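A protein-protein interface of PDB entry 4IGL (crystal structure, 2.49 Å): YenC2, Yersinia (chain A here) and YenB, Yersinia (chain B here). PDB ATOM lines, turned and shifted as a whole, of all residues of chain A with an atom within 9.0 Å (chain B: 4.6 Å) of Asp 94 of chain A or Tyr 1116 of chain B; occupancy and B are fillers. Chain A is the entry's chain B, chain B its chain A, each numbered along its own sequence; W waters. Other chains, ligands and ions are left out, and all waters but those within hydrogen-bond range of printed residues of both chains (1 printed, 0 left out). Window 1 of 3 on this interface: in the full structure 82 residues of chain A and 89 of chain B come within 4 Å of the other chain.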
ATOM      1  N   ASP A  73      19.725 -23.480  10.216  1.00  0.00           N
ATOM      2  CA  ASP A  73      18.717 -22.472  10.540  1.00  0.00           C
ATOM      3  C   ASP A  73      17.318 -23.056  10.330  1.00  0.00           C
ATOM      4  O   ASP A  73      17.172 -24.254  10.077  1.00  0.00           O
ATOM      5  CB  ASP A  73      18.908 -21.185   9.723  1.00  0.00           C
ATOM      6  CG  ASP A  73      18.750 -21.396   8.212  1.00  0.00           C
ATOM      7  OD1 ASP A  73      18.282 -22.471   7.772  1.00  0.00           O
ATOM      8  OD2 ASP A  73      19.104 -20.466   7.454  1.00  0.00           O
ATOM      9  N   ASN A  75      15.486 -22.860   7.912  1.00  0.00           N
ATOM     10  CA  ASN A  75      15.281 -23.261   6.519  1.00  0.00           C
ATOM     11  C   ASN A  75      16.161 -24.415   6.018  1.00  0.00           C
ATOM     12  O   ASN A  75      16.077 -24.797   4.849  1.00  0.00           O
ATOM     13  CB  ASN A  75      15.425 -22.062   5.585  1.00  0.00           C
ATOM     14  CG  ASN A  75      14.284 -21.082   5.724  1.00  0.00           C
ATOM     15  OD1 ASN A  75      13.190 -21.448   6.155  1.00  0.00           O
ATOM     16  ND2 ASN A  75      14.523 -19.831   5.341  1.00  0.00           N
ATOM     17  N   ASN A  77      19.523 -24.490   6.009  1.00  0.00           N
ATOM     18  CA  ASN A  77      20.865 -24.070   5.645  1.00  0.00           C
ATOM     19  C   ASN A  77      21.817 -24.397   6.781  1.00  0.00           C
ATOM     20  O   ASN A  77      21.580 -24.011   7.922  1.00  0.00           O
ATOM     21  CB  ASN A  77      20.914 -22.571   5.329  1.00  0.00           C
ATOM     22  CG  ASN A  77      20.073 -22.196   4.121  1.00  0.00           C
ATOM     23  OD1 ASN A  77      20.418 -22.528   2.983  1.00  0.00           O
ATOM     24  ND2 ASN A  77      18.977 -21.480   4.359  1.00  0.00           N
ATOM     25  N   ILE A  79      24.657 -24.166   9.329  1.00  0.00           N
ATOM     26  CA  ILE A  79      25.446 -23.126   9.980  1.00  0.00           C
ATOM     27  C   ILE A  79      26.677 -23.768  10.617  1.00  0.00           C
ATOM     28  O   ILE A  79      27.804 -23.319  10.401  1.00  0.00           O
ATOM     29  CB  ILE A  79      24.619 -22.374  11.054  1.00  0.00           C
ATOM     30  CG1 ILE A  79      23.460 -21.617  10.405  1.00  0.00           C
ATOM     31  CG2 ILE A  79      25.488 -21.397  11.831  1.00  0.00           C
ATOM     32  CD1 ILE A  79      22.614 -20.846  11.392  1.00  0.00           C
ATOM     33  N   VAL A  91      29.685 -21.581   9.242  1.00  0.00           N
ATOM     34  CA  VAL A  91      29.525 -20.645   8.134  1.00  0.00           C
ATOM     35  C   VAL A  91      28.227 -19.878   8.273  1.00  0.00           C
ATOM     36  O   VAL A  91      27.285 -20.356   8.902  1.00  0.00           O
ATOM     37  CB  VAL A  91      29.568 -21.351   6.755  1.00  0.00           C
ATOM     38  CG1 VAL A  91      30.945 -21.942   6.501  1.00  0.00           C
ATOM     39  CG2 VAL A  91      28.482 -22.418   6.657  1.00  0.00           C
ATOM     40  N   LEU A  92      28.184 -18.681   7.699  1.00  0.00           N
ATOM     41  CA  LEU A  92      26.944 -17.921   7.656  1.00  0.00           C
ATOM     42  C   LEU A  92      26.886 -17.022   6.429  1.00  0.00           C
ATOM     43  O   LEU A  92      27.879 -16.363   6.065  1.00  0.00           O
ATOM     44  CB  LEU A  92      26.753 -17.099   8.936  1.00  0.00           C
ATOM     45  CG  LEU A  92      25.363 -16.482   9.138  1.00  0.00           C
ATOM     46  CD1 LEU A  92      24.357 -17.560   9.509  1.00  0.00           C
ATOM     47  CD2 LEU A  92      25.377 -15.389  10.197  1.00  0.00           C
ATOM     48  N   ASN A  93      25.704 -17.009   5.812  1.00  0.00           N
ATOM     49  CA  ASN A  93      25.391 -16.156   4.671  1.00  0.00           C
ATOM     50  C   ASN A  93      24.440 -15.041   5.100  1.00  0.00           C
ATOM     51  O   ASN A  93      23.741 -15.168   6.111  1.00  0.00           O
ATOM     52  CB  ASN A  93      24.742 -16.964   3.538  1.00  0.00           C
ATOM     53  CG  ASN A  93      25.610 -18.116   3.058  1.00  0.00           C
ATOM     54  OD1 ASN A  93      26.544 -17.924   2.280  1.00  0.00           O
ATOM     55  ND2 ASN A  93      25.291 -19.327   3.509  1.00  0.00           N
ATOM     56  N   ASP A  94      24.410 -13.951   4.339  1.00  0.00           N
ATOM     57  CA  ASP A  94      23.507 -12.840   4.643  1.00  0.00           C
ATOM     58  C   ASP A  94      22.119 -12.981   4.008  1.00  0.00           C
ATOM     59  O   ASP A  94      21.802 -14.004   3.393  1.00  0.00           O
ATOM     60  CB  ASP A  94      24.140 -11.491   4.275  1.00  0.00           C
ATOM     61  CG  ASP A  94      24.531 -11.401   2.808  1.00  0.00           C
ATOM     62  OD1 ASP A  94      23.973 -12.161   1.985  1.00  0.00           O
ATOM     63  OD2 ASP A  94      25.402 -10.566   2.478  1.00  0.00           O
ATOM     64  N   THR A  95      21.307 -11.938   4.154  1.00  0.00           N
ATOM     65  CA  THR A  95      19.943 -11.937   3.631  1.00  0.00           C
ATOM     66  C   THR A  95      19.922 -11.819   2.110  1.00  0.00           C
ATOM     67  O   THR A  95      18.906 -12.092   1.472  1.00  0.00           O
ATOM     68  CB  THR A  95      19.117 -10.787   4.232  1.00  0.00           C
ATOM     69  OG1 THR A  95      19.761  -9.538   3.958  1.00  0.00           O
ATOM     70  CG2 THR A  95      18.982 -10.964   5.735  1.00  0.00           C
ATOM     71  N   GLU A  96      21.049 -11.413   1.536  1.00  0.00           N
ATOM     72  CA  GLU A  96      21.175 -11.300   0.090  1.00  0.00           C
ATOM     73  C   GLU A  96      21.696 -12.626  -0.457  1.00  0.00           C
ATOM     74  O   GLU A  96      21.868 -12.794  -1.664  1.00  0.00           O
ATOM     75  CB  GLU A  96      22.127 -10.155  -0.272  1.00  0.00           C
ATOM     76  CG  GLU A  96      21.971  -9.634  -1.697  1.00  0.00           C
ATOM     77  CD  GLU A  96      20.840  -8.635  -1.843  1.00  0.00           C
ATOM     78  OE1 GLU A  96      20.325  -8.160  -0.811  1.00  0.00           O
ATOM     79  OE2 GLU A  96      20.470  -8.320  -2.995  1.00  0.00           O
ATOM     80  N   GLY A  97      21.944 -13.566   0.450  1.00  0.00           N
ATOM     81  CA  GLY A  97      22.412 -14.888   0.079  1.00  0.00           C
ATOM     82  C   GLY A  97      23.921 -14.982  -0.033  1.00  0.00           C
ATOM     83  O   GLY A  97      24.456 -16.031  -0.400  1.00  0.00           O
ATOM     84  N   ARG A  98      24.605 -13.892   0.306  1.00  0.00           N
ATOM     85  CA  ARG A  98      26.059 -13.807   0.172  1.00  0.00           C
ATOM     86  C   ARG A  98      26.766 -14.342   1.415  1.00  0.00           C
ATOM     87  O   ARG A  98      26.307 -14.129   2.538  1.00  0.00           O
ATOM     88  CB  ARG A  98      26.480 -12.349  -0.059  1.00  0.00           C
ATOM     89  CG  ARG A  98      25.690 -11.624  -1.142  1.00  0.00           C
ATOM     90  CD  ARG A  98      26.068 -10.150  -1.236  1.00  0.00           C
ATOM     91  NE  ARG A  98      25.720  -9.417  -0.020  1.00  0.00           N
ATOM     92  CZ  ARG A  98      25.694  -8.090   0.081  1.00  0.00           C
ATOM     93  NH1 ARG A  98      25.361  -7.519   1.230  1.00  0.00           N
ATOM     94  NH2 ARG A  98      25.992  -7.332  -0.965  1.00  0.00           N
ATOM     95  N   SER A  99      27.893 -15.020   1.215  1.00  0.00           N
ATOM     96  CA  SER A  99      28.683 -15.513   2.337  1.00  0.00           C
ATOM     97  C   SER A  99      29.232 -14.324   3.109  1.00  0.00           C
ATOM     98  O   SER A  99      29.745 -13.374   2.515  1.00  0.00           O
ATOM     99  CB  SER A  99      29.844 -16.382   1.848  1.00  0.00           C
ATOM    100  OG  SER A  99      29.385 -17.445   1.033  1.00  0.00           O
ATOM    101  N   VAL A 100      29.113 -14.368   4.431  1.00  0.00           N
ATOM    102  CA  VAL A 100      29.642 -13.291   5.258  1.00  0.00           C
ATOM    103  C   VAL A 100      30.690 -13.812   6.235  1.00  0.00           C
ATOM    104  O   VAL A 100      31.629 -13.087   6.575  1.00  0.00           O
ATOM    105  CB  VAL A 100      28.536 -12.511   6.008  1.00  0.00           C
ATOM    106  CG1 VAL A 100      27.643 -11.787   5.022  1.00  0.00           C
ATOM    107  CG2 VAL A 100      27.719 -13.436   6.886  1.00  0.00           C
ATOM    108  N   ILE A 101      30.562 -15.064   6.676  1.00  0.00           N
ATOM    109  CA  ILE A 101      31.599 -15.602   7.567  1.00  0.00           C
ATOM    110  C   ILE A 101      31.853 -17.112   7.416  1.00  0.00           C
ATOM    111  O   ILE A 101      30.933 -17.888   7.141  1.00  0.00           O
ATOM    112  CB  ILE A 101      31.316 -15.239   9.059  1.00  0.00           C
ATOM    113  CG1 ILE A 101      32.543 -15.520   9.941  1.00  0.00           C
ATOM    114  CG2 ILE A 101      30.072 -15.950   9.567  1.00  0.00           C
ATOM    115  CD1 ILE A 101      32.332 -15.233  11.420  1.00  0.00           C
ATOM    116  N   PHE A 124      33.747 -11.817   4.744  1.00  0.00           N
ATOM    117  CA  PHE A 124      33.569 -11.236   3.421  1.00  0.00           C
ATOM    118  C   PHE A 124      32.841  -9.899   3.543  1.00  0.00           C
ATOM    119  O   PHE A 124      31.803  -9.799   4.200  1.00  0.00           O
ATOM    120  CB  PHE A 124      32.796 -12.218   2.529  1.00  0.00           C
ATOM    121  CG  PHE A 124      33.379 -13.622   2.522  1.00  0.00           C
ATOM    122  CD1 PHE A 124      33.043 -14.539   3.516  1.00  0.00           C
ATOM    123  CD2 PHE A 124      34.249 -14.026   1.515  1.00  0.00           C
ATOM    124  CE1 PHE A 124      33.575 -15.824   3.513  1.00  0.00           C
ATOM    125  CE2 PHE A 124      34.781 -15.309   1.502  1.00  0.00           C
ATOM    126  CZ  PHE A 124      34.444 -16.209   2.503  1.00  0.00           C
ATOM    127  N   GLN A 125      33.394  -8.873   2.904  1.00  0.00           N
ATOM    128  CA  GLN A 125      32.835  -7.528   2.975  1.00  0.00           C
ATOM    129  C   GLN A 125      32.345  -7.094   1.605  1.00  0.00           C
ATOM    130  O   GLN A 125      32.996  -7.351   0.584  1.00  0.00           O
ATOM    131  CB  GLN A 125      33.872  -6.529   3.508  1.00  0.00           C
ATOM    132  CG  GLN A 125      34.365  -6.822   4.920  1.00  0.00           C
ATOM    133  CD  GLN A 125      35.449  -7.887   4.955  1.00  0.00           C
ATOM    134  OE1 GLN A 125      35.446  -8.763   5.822  1.00  0.00           O
ATOM    135  NE2 GLN A 125      36.384  -7.814   4.014  1.00  0.00           N
ATOM    136  N   TYR A 126      31.204  -6.413   1.593  1.00  0.00           N
ATOM    137  CA  TYR A 126      30.562  -6.007   0.349  1.00  0.00           C
ATOM    138  C   TYR A 126      30.326  -4.504   0.317  1.00  0.00           C
ATOM    139  O   TYR A 126      30.361  -3.840   1.358  1.00  0.00           O
ATOM    140  CB  TYR A 126      29.242  -6.769   0.175  1.00  0.00           C
ATOM    141  CG  TYR A 126      29.420  -8.269   0.233  1.00  0.00           C
ATOM    142  CD1 TYR A 126      29.762  -8.986  -0.906  1.00  0.00           C
ATOM    143  CD2 TYR A 126      29.290  -8.963   1.428  1.00  0.00           C
ATOM    144  CE1 TYR A 126      29.944 -10.348  -0.865  1.00  0.00           C
ATOM    145  CE2 TYR A 126      29.473 -10.329   1.481  1.00  0.00           C
ATOM    146  CZ  TYR A 126      29.801 -11.017   0.328  1.00  0.00           C
ATOM    147  OH  TYR A 126      29.983 -12.382   0.357  1.00  0.00           O
ATOM    148  N   GLU A 127      30.116  -3.971  -0.885  1.00  0.00           N
ATOM    149  CA  GLU A 127      29.771  -2.567  -1.042  1.00  0.00           C
ATOM    150  C   GLU A 127      28.564  -2.275  -0.169  1.00  0.00           C
ATOM    151  O   GLU A 127      27.605  -3.044  -0.148  1.00  0.00           O
ATOM    152  CB  GLU A 127      29.404  -2.252  -2.495  1.00  0.00           C
ATOM    153  CG  GLU A 127      30.555  -2.215  -3.476  1.00  0.00           C
ATOM    154  CD  GLU A 127      30.080  -1.935  -4.893  1.00  0.00           C
ATOM    155  OE1 GLU A 127      28.961  -2.365  -5.243  1.00  0.00           O
ATOM    156  OE2 GLU A 127      30.816  -1.269  -5.652  1.00  0.00           O
ATOM    157  N   GLY A 133      26.086  -3.413  -3.683  1.00  0.00           N
ATOM    158  CA  GLY A 133      26.520  -4.438  -2.756  1.00  0.00           C
ATOM    159  C   GLY A 133      27.413  -5.481  -3.393  1.00  0.00           C
ATOM    160  O   GLY A 133      27.378  -6.657  -3.013  1.00  0.00           O
ATOM    161  N   ARG A 134      28.225  -5.053  -4.356  1.00  0.00           N
ATOM    162  CA  ARG A 134      29.193  -5.948  -4.983  1.00  0.00           C
ATOM    163  C   ARG A 134      30.263  -6.341  -3.965  1.00  0.00           C
ATOM    164  O   ARG A 134      30.442  -5.657  -2.955  1.00  0.00           O
ATOM    165  CB  ARG A 134      29.828  -5.268  -6.205  1.00  0.00           C
ATOM    166  CG  ARG A 134      28.945  -5.273  -7.451  1.00  0.00           C
ATOM    167  CD  ARG A 134      29.410  -4.250  -8.484  1.00  0.00           C
ATOM    168  NE  ARG A 134      29.540  -2.917  -7.895  1.00  0.00           N
ATOM    169  CZ  ARG A 134      29.715  -1.793  -8.586  1.00  0.00           C
ATOM    170  NH1 ARG A 134      29.773  -1.821  -9.911  1.00  0.00           N
ATOM    171  NH2 ARG A 134      29.821  -0.635  -7.946  1.00  0.00           N
ATOM    172  N   ILE B1089      14.352 -17.056  10.353  1.00  0.00           N
ATOM    173  CA  ILE B1089      15.576 -17.785  10.032  1.00  0.00           C
ATOM    174  C   ILE B1089      16.106 -18.484  11.275  1.00  0.00           C
ATOM    175  O   ILE B1089      16.515 -19.648  11.227  1.00  0.00           O
ATOM    176  CB  ILE B1089      16.682 -16.836   9.534  1.00  0.00           C
ATOM    177  CG1 ILE B1089      16.127 -15.876   8.479  1.00  0.00           C
ATOM    178  CG2 ILE B1089      17.843 -17.631   8.946  1.00  0.00           C
ATOM    179  CD1 ILE B1089      15.586 -16.575   7.248  1.00  0.00           C
ATOM    180  N   LEU B1111      24.922 -11.337  13.154  1.00  0.00           N
ATOM    181  CA  LEU B1111      23.591 -11.447  12.569  1.00  0.00           C
ATOM    182  C   LEU B1111      23.087 -10.083  12.109  1.00  0.00           C
ATOM    183  O   LEU B1111      22.570  -9.945  11.001  1.00  0.00           O
ATOM    184  CB  LEU B1111      22.616 -12.065  13.576  1.00  0.00           C
ATOM    185  CG  LEU B1111      22.766 -13.571  13.831  1.00  0.00           C
ATOM    186  CD1 LEU B1111      21.922 -14.037  15.009  1.00  0.00           C
ATOM    187  CD2 LEU B1111      22.408 -14.352  12.581  1.00  0.00           C
ATOM    188  N   PHE B1112      23.261  -9.077  12.961  1.00  0.00           N
ATOM    189  CA  PHE B1112      22.863  -7.713  12.637  1.00  0.00           C
ATOM    190  C   PHE B1112      23.605  -7.222  11.400  1.00  0.00           C
ATOM    191  O   PHE B1112      23.014  -6.597  10.522  1.00  0.00           O
ATOM    192  CB  PHE B1112      23.144  -6.777  13.819  1.00  0.00           C
ATOM    193  CG  PHE B1112      22.009  -6.673  14.808  1.00  0.00           C
ATOM    194  CD1 PHE B1112      20.693  -6.600  14.370  1.00  0.00           C
ATOM    195  CD2 PHE B1112      22.260  -6.643  16.174  1.00  0.00           C
ATOM    196  CE1 PHE B1112      19.646  -6.503  15.277  1.00  0.00           C
ATOM    197  CE2 PHE B1112      21.217  -6.544  17.089  1.00  0.00           C
ATOM    198  CZ  PHE B1112      19.909  -6.474  16.638  1.00  0.00           C
ATOM    199  N   ALA B1114      24.689  -9.018   9.051  1.00  0.00           N
ATOM    200  CA  ALA B1114      24.317  -9.837   7.904  1.00  0.00           C
ATOM    201  C   ALA B1114      22.888  -9.590   7.412  1.00  0.00           C
ATOM    202  O   ALA B1114      22.366 -10.343   6.588  1.00  0.00           O
ATOM    203  CB  ALA B1114      24.532 -11.311   8.215  1.00  0.00           C
ATOM    204  N   GLY B1115      22.258  -8.533   7.916  1.00  0.00           N
ATOM    205  CA  GLY B1115      20.958  -8.129   7.413  1.00  0.00           C
ATOM    206  C   GLY B1115      19.772  -8.706   8.157  1.00  0.00           C
ATOM    207  O   GLY B1115      18.625  -8.433   7.811  1.00  0.00           O
ATOM    208  N   TYR B1116      20.036  -9.517   9.172  1.00  0.00           N
ATOM    209  CA  TYR B1116      18.952 -10.096   9.949  1.00  0.00           C
ATOM    210  C   TYR B1116      18.520  -9.137  11.049  1.00  0.00           C
ATOM    211  O   TYR B1116      19.313  -8.313  11.513  1.00  0.00           O
ATOM    212  CB  TYR B1116      19.372 -11.440  10.537  1.00  0.00           C
ATOM    213  CG  TYR B1116      19.873 -12.416   9.500  1.00  0.00           C
ATOM    214  CD1 TYR B1116      18.990 -13.065   8.646  1.00  0.00           C
ATOM    215  CD2 TYR B1116      21.231 -12.681   9.368  1.00  0.00           C
ATOM    216  CE1 TYR B1116      19.444 -13.960   7.696  1.00  0.00           C
ATOM    217  CE2 TYR B1116      21.693 -13.571   8.420  1.00  0.00           C
ATOM    218  CZ  TYR B1116      20.794 -14.208   7.588  1.00  0.00           C
ATOM    219  OH  TYR B1116      21.253 -15.096   6.643  1.00  0.00           O
ATOM    220  N   GLN B1117      17.262  -9.246  11.459  1.00  0.00           N
ATOM    221  CA  GLN B1117      16.722  -8.390  12.510  1.00  0.00           C
ATOM    222  C   GLN B1117      15.707  -9.152  13.345  1.00  0.00           C
ATOM    223  O   GLN B1117      15.190 -10.183  12.917  1.00  0.00           O
ATOM    224  CB  GLN B1117      16.086  -7.138  11.903  1.00  0.00           C
ATOM    225  CG  GLN B1117      15.070  -7.432  10.816  1.00  0.00           C
ATOM    226  CD  GLN B1117      14.330  -6.193  10.354  1.00  0.00           C
ATOM    227  OE1 GLN B1117      14.584  -5.676   9.264  1.00  0.00           O
ATOM    228  NE2 GLN B1117      13.407  -5.712  11.179  1.00  0.00           N
ATOM    229  N   TRP B1132      14.797 -14.185  14.828  1.00  0.00           N
ATOM    230  CA  TRP B1132      15.583 -13.457  13.846  1.00  0.00           C
ATOM    231  C   TRP B1132      14.952 -13.666  12.482  1.00  0.00           C
ATOM    232  O   TRP B1132      14.730 -14.801  12.070  1.00  0.00           O
ATOM    233  CB  TRP B1132      17.021 -13.965  13.862  1.00  0.00           C
ATOM    234  CG  TRP B1132      17.765 -13.516  15.076  1.00  0.00           C
ATOM    235  CD1 TRP B1132      17.907 -14.197  16.249  1.00  0.00           C
ATOM    236  CD2 TRP B1132      18.493 -12.296  15.227  1.00  0.00           C
ATOM    237  NE1 TRP B1132      18.664 -13.465  17.130  1.00  0.00           N
ATOM    238  CE2 TRP B1132      19.040 -12.294  16.526  1.00  0.00           C
ATOM    239  CE3 TRP B1132      18.733 -11.200  14.392  1.00  0.00           C
ATOM    240  CZ2 TRP B1132      19.809 -11.238  17.012  1.00  0.00           C
ATOM    241  CZ3 TRP B1132      19.496 -10.153  14.873  1.00  0.00           C
ATOM    242  CH2 TRP B1132      20.026 -10.179  16.172  1.00  0.00           C
ATOM    243  N   VAL B1133      14.664 -12.581  11.776  1.00  0.00           N
ATOM    244  CA  VAL B1133      13.976 -12.702  10.497  1.00  0.00           C
ATOM    245  C   VAL B1133      14.767 -12.035   9.387  1.00  0.00           C
ATOM    246  O   VAL B1133      15.690 -11.255   9.636  1.00  0.00           O
ATOM    247  CB  VAL B1133      12.556 -12.069  10.539  1.00  0.00           C
ATOM    248  CG1 VAL B1133      11.649 -12.822  11.505  1.00  0.00           C
ATOM    249  CG2 VAL B1133      12.635 -10.598  10.916  1.00  0.00           C
ATOM    250  N   ALA B1134      14.389 -12.345   8.156  1.00  0.00           N
ATOM    251  CA  ALA B1134      14.959 -11.690   6.996  1.00  0.00           C
ATOM    252  C   ALA B1134      13.833 -11.060   6.201  1.00  0.00           C
ATOM    253  O   ALA B1134      12.810 -11.698   5.927  1.00  0.00           O
ATOM    254  CB  ALA B1134      15.727 -12.678   6.141  1.00  0.00           C
ATOM    255  N   LEU B1158      20.338  -4.036   2.180  1.00  0.00           N
ATOM    256  CA  LEU B1158      21.792  -4.117   2.151  1.00  0.00           C
ATOM    257  C   LEU B1158      22.326  -3.560   0.830  1.00  0.00           C
ATOM    258  O   LEU B1158      23.495  -3.176   0.736  1.00  0.00           O
ATOM    259  CB  LEU B1158      22.253  -5.570   2.312  1.00  0.00           C
ATOM    260  CG  LEU B1158      21.947  -6.324   3.609  1.00  0.00           C
ATOM    261  CD1 LEU B1158      22.536  -7.725   3.567  1.00  0.00           C
ATOM    262  CD2 LEU B1158      22.466  -5.571   4.822  1.00  0.00           C
HETATM  263  O   HOH W   1      21.280 -18.314   7.677  1.00  0.00           O
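O of Trp 1132 of chain B lies within hydrogen-bond range of N of Ile 1089 of chain B (2.9 Å).
N of Val 100 of chain A is in hydrogen-bond range of O of Leu 92 of chain A (2.9 Å).
The backbone carbonyl oxygen (O) of Ile 101 of chain A is in hydrogen-bond range of the backbone NH (N) of Leu 92 of chain A.
The side-chain carboxylate (OD1) of Asp 94 of chain A lies within hydrogen-bond range of the backbone NH (N) of Glu 96 of chain A, at 3.1 Å.
OD1 of Asp 94 of chain A is in hydrogen-bond range of N of Gly 97 of chain A, 2.9 Å away.
OD2 of Asp 94 of chain A is in salt-bridge range of NE of Arg 98 of chain A.
Water W1 bridges OD2 of Asp 73 of chain A and OH of Tyr 1116 of chain B.
Printed residues of chain A that touch a printed residue of chain B: Asp 73, Asn 75, Leu 92, Asn 93, Asp 94, Thr 95 and Arg 98.
N of Thr 95 of chain A sits at hydrogen-bond distance from O of Ala 1114 of chain B (3.1 Å).
O of Asn 93 of chain A lies within hydrogen-bond range of OH of Tyr 1116 of chain B, 2.5 Å away.
The side-chain hydroxyl (OH) of Tyr 1116 of chain B is in hydrogen-bond range of the backbone carbonyl oxygen (O) of Asp 94 of chain A, 3.5 Å away.
Asp 73 of chain A touches Ile 1089 of chain B.
Asn 75 of chain A touches Ile 1089 of chain B (ND2 to CD1, 3.9 Å).
CD2 of Leu 1111 of chain B touches CD2 of Leu 92 of chain A (3.9 Å).
Asp 94 of chain A touches Ala 1114 of chain B.
CG2 of Thr 95 of chain A touches O of Gly 1115 of chain B, at 3.3 Å.
Thr 95 of chain A touches Tyr 1116 of chain B.
Ala 1134 of chain B touches Thr 95 of chain A (CB to CG2, 3.7 Å).
Thr 95 of chain A touches Leu 1158 of chain B.
Leu 1158 of chain B touches Arg 98 of chain A (CD1 to NH1, 3.7 Å).
Asp 94 of chain A touches just these residues of chain B: Ala 1114 (3.1 Å) and Tyr 1116 (3.5 Å).
Tyr 1116 of chain B touches just these residues of chain A: Asn 93, Asp 94 and Thr 95.
Of the printed residues of chain A, Gly 1115 of chain B touches Thr 95.
Printed residues of chain B within 4 Å of Asp 73 of chain A: Ile 1089 (3.2 Å).
Printed residues of chain B within 4 Å of Thr 95 of chain A: Ala 1114 (3.1 Å), Gly 1115 (3.3 Å), Tyr 1116 (3.6 Å), Ala 1134 (3.7 Å) and Leu 1158 (3.3 Å).
Printed residues of chain B within 4 Å of Leu 92 of chain A: Leu 1111.
The nearest residue of chain B that does not touch Asp 94 of chain A is Leu 1158 of chain B (4.2 Å).
The nearest residue of chain A that does not touch Tyr 1116 of chain B is Leu 92 of chain A (4.5 Å).
The nearest printed residue of chain B that does not touch Asp 73 of chain A is Tyr 1116 of chain B (5.8 Å).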
